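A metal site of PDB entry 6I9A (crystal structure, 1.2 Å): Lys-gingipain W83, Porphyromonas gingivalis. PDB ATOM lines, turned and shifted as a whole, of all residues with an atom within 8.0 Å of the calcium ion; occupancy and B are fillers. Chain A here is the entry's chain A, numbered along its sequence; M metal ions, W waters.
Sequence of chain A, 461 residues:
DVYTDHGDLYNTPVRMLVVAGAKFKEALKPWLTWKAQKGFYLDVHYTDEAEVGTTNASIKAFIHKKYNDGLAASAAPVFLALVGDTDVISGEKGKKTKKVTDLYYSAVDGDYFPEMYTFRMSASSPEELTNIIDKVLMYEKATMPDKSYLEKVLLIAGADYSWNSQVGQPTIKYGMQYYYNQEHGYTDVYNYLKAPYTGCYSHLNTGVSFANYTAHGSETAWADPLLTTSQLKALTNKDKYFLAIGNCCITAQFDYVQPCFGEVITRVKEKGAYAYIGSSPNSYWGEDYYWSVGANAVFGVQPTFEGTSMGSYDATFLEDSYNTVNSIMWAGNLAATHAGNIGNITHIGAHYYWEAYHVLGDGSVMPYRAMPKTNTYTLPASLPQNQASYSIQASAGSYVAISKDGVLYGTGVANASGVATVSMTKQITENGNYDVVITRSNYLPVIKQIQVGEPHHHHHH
The side-chain carboxylate (OE2) of Glu 263 lies close to the guanidinium group (NH2) of Arg 267, 3.5 Å away.
The side-chain carboxylate (OE2) of Glu 263 sits close to the side-chain hydroxyl (OG) of Ser 122, at 2.6 Å.
The side-chain carboxylate of Asp 85 lies close to the guanidinium group of Arg 267 (2.8 Å).
The backbone NH of Glu 263 sits at hydrogen-bond distance from the side-chain sulfur of Cys 260, at 3.6 Å.
The guanidinium group of Arg 120 sits close to the backbone carbonyl oxygen of Asp 85, at 3.4 Å.
The nearest printed residue that does not touch the calcium ion is Asp 255 (4.4 Å).
The calcium ion is bound by the backbone carbonyl oxygen (O) of Phe 254 (2.3 Å), water W3 (2.4 Å), water W2 (2.4 Å), water W1 (2.5 Å), the side-chain carboxylate (OE2) of Glu 263 (2.5 Å), the side-chain carboxylate (OD1) of Asp 85 (2.5 Å), the side-chain carboxylate (OD2) of Asp 85 (2.5 Å) and the side-chain carboxylate (OE1) of Glu 263 (2.6 Å).
The calcium ion has eight donor atoms within binding distance.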
ATOM      1  N   GLY A  84       8.573   9.712  28.255  1.00  0.00           N
ATOM      2  CA  GLY A  84       7.538  10.417  27.515  1.00  0.00           C
ATOM      3  C   GLY A  84       8.095  11.240  26.378  1.00  0.00           C
ATOM      4  O   GLY A  84       9.312  11.497  26.307  1.00  0.00           O
ATOM      5  N   ASP A  85       7.208  11.622  25.497  1.00  0.00           N
ATOM      6  CA  ASP A  85       7.514  12.494  24.385  1.00  0.00           C
ATOM      7  C   ASP A  85       7.298  13.972  24.836  1.00  0.00           C
ATOM      8  O   ASP A  85       7.065  14.266  26.001  1.00  0.00           O
ATOM      9  CB  ASP A  85       6.683  12.083  23.151  1.00  0.00           C
ATOM     10  CG  ASP A  85       7.235  12.508  21.783  1.00  0.00           C
ATOM     11  OD1 ASP A  85       8.107  13.431  21.723  1.00  0.00           O
ATOM     12  OD2 ASP A  85       6.828  11.906  20.768  1.00  0.00           O
ATOM     13  N   THR A  86       7.407  14.878  23.871  1.00  0.00           N
ATOM     14  CA  THR A  86       7.386  16.334  24.156  1.00  0.00           C
ATOM     15  C   THR A  86       6.021  16.837  24.536  1.00  0.00           C
ATOM     16  O   THR A  86       5.937  17.939  25.062  1.00  0.00           O
ATOM     17  CB  THR A  86       7.978  17.113  22.978  1.00  0.00           C
ATOM     18  OG1 THR A  86       7.228  16.834  21.808  1.00  0.00           O
ATOM     19  CG2 THR A  86       9.465  16.768  22.763  1.00  0.00           C
ATOM     20  N   ASP A  87       4.975  16.036  24.367  1.00  0.00           N
ATOM     21  CA  ASP A  87       3.628  16.430  24.821  1.00  0.00           C
ATOM     22  C   ASP A  87       3.556  16.376  26.360  1.00  0.00           C
ATOM     23  O   ASP A  87       2.650  16.988  26.940  1.00  0.00           O
ATOM     24  CB  ASP A  87       2.563  15.521  24.221  1.00  0.00           C
ATOM     25  CG  ASP A  87       2.659  14.039  24.467  1.00  0.00           C
ATOM     26  OD1 ASP A  87       3.795  13.530  24.774  1.00  0.00           O
ATOM     27  OD2 ASP A  87       1.627  13.371  24.369  1.00  0.00           O
ATOM     28  N   VAL A 100      15.110  21.483  19.723  1.00  0.00           N
ATOM     29  CA  VAL A 100      14.795  20.938  21.050  1.00  0.00           C
ATOM     30  C   VAL A 100      16.036  20.286  21.653  1.00  0.00           C
ATOM     31  O   VAL A 100      16.848  19.626  20.974  1.00  0.00           O
ATOM     32  CB  VAL A 100      13.586  19.971  20.969  1.00  0.00           C
ATOM     33  CG1 VAL A 100      13.926  18.661  20.224  1.00  0.00           C
ATOM     34  CG2 VAL A 100      13.011  19.700  22.368  1.00  0.00           C
ATOM     35  N   ARG A 120      16.066   9.722  27.218  1.00  0.00           N
ATOM     36  CA  ARG A 120      14.640   9.871  27.077  1.00  0.00           C
ATOM     37  C   ARG A 120      14.025   8.637  26.451  1.00  0.00           C
ATOM     38  O   ARG A 120      14.346   8.279  25.317  1.00  0.00           O
ATOM     39  CB  ARG A 120      14.293  11.129  26.257  1.00  0.00           C
ATOM     40  CG  ARG A 120      12.799  11.287  25.949  1.00  0.00           C
ATOM     41  CD  ARG A 120      12.533  12.490  25.065  1.00  0.00           C
ATOM     42  NE  ARG A 120      12.736  13.766  25.738  1.00  0.00           N
ATOM     43  CZ  ARG A 120      11.745  14.585  26.087  1.00  0.00           C
ATOM     44  NH1 ARG A 120      10.465  14.179  26.035  1.00  0.00           N
ATOM     45  NH2 ARG A 120      12.020  15.798  26.534  1.00  0.00           N
ATOM     46  N   SER A 122      11.223   7.926  24.864  1.00  0.00           N
ATOM     47  CA  SER A 122      10.139   8.667  24.205  1.00  0.00           C
ATOM     48  C   SER A 122       9.114   7.707  23.633  1.00  0.00           C
ATOM     49  O   SER A 122       9.446   6.884  22.753  1.00  0.00           O
ATOM     50  CB  SER A 122      10.692   9.555  23.099  1.00  0.00           C
ATOM     51  OG  SER A 122       9.555  10.185  22.529  1.00  0.00           O
ATOM     52  N   ALA A 123       7.877   7.829  24.096  1.00  0.00           N
ATOM     53  CA  ALA A 123       6.783   6.971  23.664  1.00  0.00           C
ATOM     54  C   ALA A 123       5.541   7.813  23.523  1.00  0.00           C
ATOM     55  O   ALA A 123       5.369   8.760  24.306  1.00  0.00           O
ATOM     56  CB  ALA A 123       6.549   5.864  24.680  1.00  0.00           C
ATOM     57  N   SER A 124       4.632   7.420  22.611  1.00  0.00           N
ATOM     58  CA  SER A 124       3.363   8.105  22.465  1.00  0.00           C
ATOM     59  C   SER A 124       2.217   7.311  23.066  1.00  0.00           C
ATOM     60  O   SER A 124       1.064   7.774  23.041  1.00  0.00           O
ATOM     61  CB  SER A 124       3.087   8.375  20.990  1.00  0.00           C
ATOM     62  OG  SER A 124       2.825   7.190  20.252  1.00  0.00           O
ATOM     63  N   ALA A 252      17.538  12.782  15.649  1.00  0.00           N
ATOM     64  CA  ALA A 252      17.026  12.739  17.019  1.00  0.00           C
ATOM     65  C   ALA A 252      16.274  14.019  17.312  1.00  0.00           C
ATOM     66  O   ALA A 252      16.149  14.412  18.464  1.00  0.00           O
ATOM     67  CB  ALA A 252      18.165  12.502  18.007  1.00  0.00           C
ATOM     68  N   GLN A 253      15.674  14.658  16.297  1.00  0.00           N
ATOM     69  CA  GLN A 253      14.869  15.906  16.527  1.00  0.00           C
ATOM     70  C   GLN A 253      13.485  15.465  16.998  1.00  0.00           C
ATOM     71  O   GLN A 253      12.519  15.379  16.235  1.00  0.00           O
ATOM     72  CB  GLN A 253      14.817  16.719  15.246  1.00  0.00           C
ATOM     73  CG  GLN A 253      14.406  18.176  15.557  1.00  0.00           C
ATOM     74  CD  GLN A 253      14.456  19.029  14.326  1.00  0.00           C
ATOM     75  OE1 GLN A 253      13.393  19.437  13.776  1.00  0.00           O
ATOM     76  NE2 GLN A 253      15.656  19.330  13.888  1.00  0.00           N
ATOM     77  N   PHE A 254      13.397  15.238  18.315  1.00  0.00           N
ATOM     78  CA  PHE A 254      12.264  14.504  18.869  1.00  0.00           C
ATOM     79  C   PHE A 254      11.039  15.355  19.144  1.00  0.00           C
ATOM     80  O   PHE A 254      10.033  14.794  19.634  1.00  0.00           O
ATOM     81  CB  PHE A 254      12.712  13.702  20.121  1.00  0.00           C
ATOM     82  CG  PHE A 254      13.313  14.552  21.197  1.00  0.00           C
ATOM     83  CD1 PHE A 254      14.701  14.687  21.318  1.00  0.00           C
ATOM     84  CD2 PHE A 254      12.513  15.193  22.123  1.00  0.00           C
ATOM     85  CE1 PHE A 254      15.261  15.492  22.307  1.00  0.00           C
ATOM     86  CE2 PHE A 254      13.057  16.014  23.113  1.00  0.00           C
ATOM     87  CZ  PHE A 254      14.436  16.152  23.231  1.00  0.00           C
ATOM     88  N   ASP A 255      11.020  16.646  18.766  1.00  0.00           N
ATOM     89  CA  ASP A 255       9.787  17.433  18.733  1.00  0.00           C
ATOM     90  C   ASP A 255       9.317  17.670  17.279  1.00  0.00           C
ATOM     91  O   ASP A 255       8.425  18.515  17.062  1.00  0.00           O
ATOM     92  CB  ASP A 255       9.992  18.767  19.448  1.00  0.00           C
ATOM     93  CG  ASP A 255      10.777  19.764  18.660  1.00  0.00           C
ATOM     94  OD1 ASP A 255      11.553  19.335  17.768  1.00  0.00           O
ATOM     95  OD2 ASP A 255      10.620  20.992  18.907  1.00  0.00           O
ATOM     96  N   TYR A 256       9.795  16.898  16.331  1.00  0.00           N
ATOM     97  CA  TYR A 256       9.368  17.007  14.951  1.00  0.00           C
ATOM     98  C   TYR A 256       7.867  16.666  14.825  1.00  0.00           C
ATOM     99  O   TYR A 256       7.295  15.976  15.686  1.00  0.00           O
ATOM    100  CB  TYR A 256      10.208  16.084  14.083  1.00  0.00           C
ATOM    101  CG  TYR A 256       9.969  16.213  12.591  1.00  0.00           C
ATOM    102  CD1 TYR A 256      10.145  17.443  11.932  1.00  0.00           C
ATOM    103  CD2 TYR A 256       9.708  15.088  11.811  1.00  0.00           C
ATOM    104  CE1 TYR A 256      10.026  17.543  10.536  1.00  0.00           C
ATOM    105  CE2 TYR A 256       9.563  15.187  10.428  1.00  0.00           C
ATOM    106  CZ  TYR A 256       9.687  16.419   9.808  1.00  0.00           C
ATOM    107  OH  TYR A 256       9.504  16.484   8.439  1.00  0.00           O
ATOM    108  N   VAL A 257       7.244  17.119  13.733  1.00  0.00           N
ATOM    109  CA  VAL A 257       5.804  16.938  13.472  1.00  0.00           C
ATOM    110  C   VAL A 257       5.440  15.457  13.333  1.00  0.00           C
ATOM    111  O   VAL A 257       4.271  15.098  13.494  1.00  0.00           O
ATOM    112  CB  VAL A 257       5.341  17.768  12.239  1.00  0.00           C
ATOM    113  CG1 VAL A 257       6.018  17.302  10.953  1.00  0.00           C
ATOM    114  CG2 VAL A 257       3.818  17.786  12.100  1.00  0.00           C
ATOM    115  N   GLN A 258       6.431  14.610  13.031  1.00  0.00           N
ATOM    116  CA  GLN A 258       6.278  13.162  12.986  1.00  0.00           C
ATOM    117  C   GLN A 258       7.285  12.559  13.966  1.00  0.00           C
ATOM    118  O   GLN A 258       8.297  13.197  14.243  1.00  0.00           O
ATOM    119  CB  GLN A 258       6.535  12.610  11.563  1.00  0.00           C
ATOM    120  CG  GLN A 258       5.546  13.147  10.486  1.00  0.00           C
ATOM    121  CD  GLN A 258       4.080  12.849  10.753  1.00  0.00           C
ATOM    122  OE1 GLN A 258       3.197  13.592  10.324  1.00  0.00           O
ATOM    123  NE2 GLN A 258       3.779  11.777  11.460  1.00  0.00           N
ATOM    124  N   PRO A 259       7.107  11.329  14.445  1.00  0.00           N
ATOM    125  CA  PRO A 259       8.160  10.717  15.261  1.00  0.00           C
ATOM    126  C   PRO A 259       9.484  10.707  14.473  1.00  0.00           C
ATOM    127  O   PRO A 259       9.534  10.374  13.272  1.00  0.00           O
ATOM    128  CB  PRO A 259       7.649   9.277  15.496  1.00  0.00           C
ATOM    129  CG  PRO A 259       6.112   9.492  15.471  1.00  0.00           C
ATOM    130  CD  PRO A 259       5.948  10.429  14.310  1.00  0.00           C
ATOM    131  N   CYS A 260      10.551  11.126  15.132  1.00  0.00           N
ATOM    132  CA  CYS A 260      11.814  11.172  14.417  1.00  0.00           C
ATOM    133  C   CYS A 260      12.409   9.761  14.291  1.00  0.00           C
ATOM    134  O   CYS A 260      11.960   8.815  14.949  1.00  0.00           O
ATOM    135  CB  CYS A 260      12.778  12.147  15.089  1.00  0.00           C
ATOM    136  SG  CYS A 260      13.383  11.610  16.729  1.00  0.00           S
ATOM    137  N   GLU A 263      13.217   8.074  17.552  1.00  0.00           N
ATOM    138  CA  GLU A 263      12.036   7.624  18.271  1.00  0.00           C
ATOM    139  C   GLU A 263      11.520   6.345  17.618  1.00  0.00           C
ATOM    140  O   GLU A 263      11.161   5.388  18.296  1.00  0.00           O
ATOM    141  CB  GLU A 263      10.955   8.721  18.252  1.00  0.00           C
ATOM    142  CG  GLU A 263      11.283   9.833  19.244  1.00  0.00           C
ATOM    143  CD  GLU A 263      10.325  11.009  19.161  1.00  0.00           C
ATOM    144  OE1 GLU A 263      10.072  11.530  18.057  1.00  0.00           O
ATOM    145  OE2 GLU A 263       9.888  11.463  20.245  1.00  0.00           O
ATOM    146  N   ARG A 267      10.979   2.780  19.388  1.00  0.00           N
ATOM    147  CA  ARG A 267       9.566   2.415  19.644  1.00  0.00           C
ATOM    148  C   ARG A 267       9.136   1.131  18.942  1.00  0.00           C
ATOM    149  O   ARG A 267       8.181   0.516  19.403  1.00  0.00           O
ATOM    150  CB  ARG A 267       8.642   3.536  19.179  1.00  0.00           C
ATOM    151  CG  ARG A 267       8.734   4.792  20.011  1.00  0.00           C
ATOM    152  CD  ARG A 267       7.946   5.896  19.357  1.00  0.00           C
ATOM    153  NE  ARG A 267       8.006   7.065  20.227  1.00  0.00           N
ATOM    154  CZ  ARG A 267       7.265   8.161  20.066  1.00  0.00           C
ATOM    155  NH1 ARG A 267       6.445   8.273  19.009  1.00  0.00           N
ATOM    156  NH2 ARG A 267       7.381   9.178  20.910  1.00  0.00           N
ATOM    157  N   LEU A 360      17.999   8.446  22.998  1.00  0.00           N
ATOM    158  CA  LEU A 360      16.594   7.994  22.977  1.00  0.00           C
ATOM    159  C   LEU A 360      16.614   6.488  23.275  1.00  0.00           C
ATOM    160  O   LEU A 360      17.519   5.765  22.842  1.00  0.00           O
ATOM    161  CB  LEU A 360      15.937   8.288  21.626  1.00  0.00           C
ATOM    162  CG  LEU A 360      15.723   9.789  21.398  1.00  0.00           C
ATOM    163  CD1 LEU A 360      15.564  10.123  19.909  1.00  0.00           C
ATOM    164  CD2 LEU A 360      14.478  10.273  22.177  1.00  0.00           C
HETATM  165 CA    CA M   1       8.389  13.161  19.257  1.00  0.00          CA
HETATM  166  O   HOH W   1       8.814  14.057  17.016  1.00  0.00           O
HETATM  167  O   HOH W   2       6.948  15.086  19.584  1.00  0.00           O
HETATM  168  O   HOH W   3       6.701  12.225  17.891  1.00  0.00           O
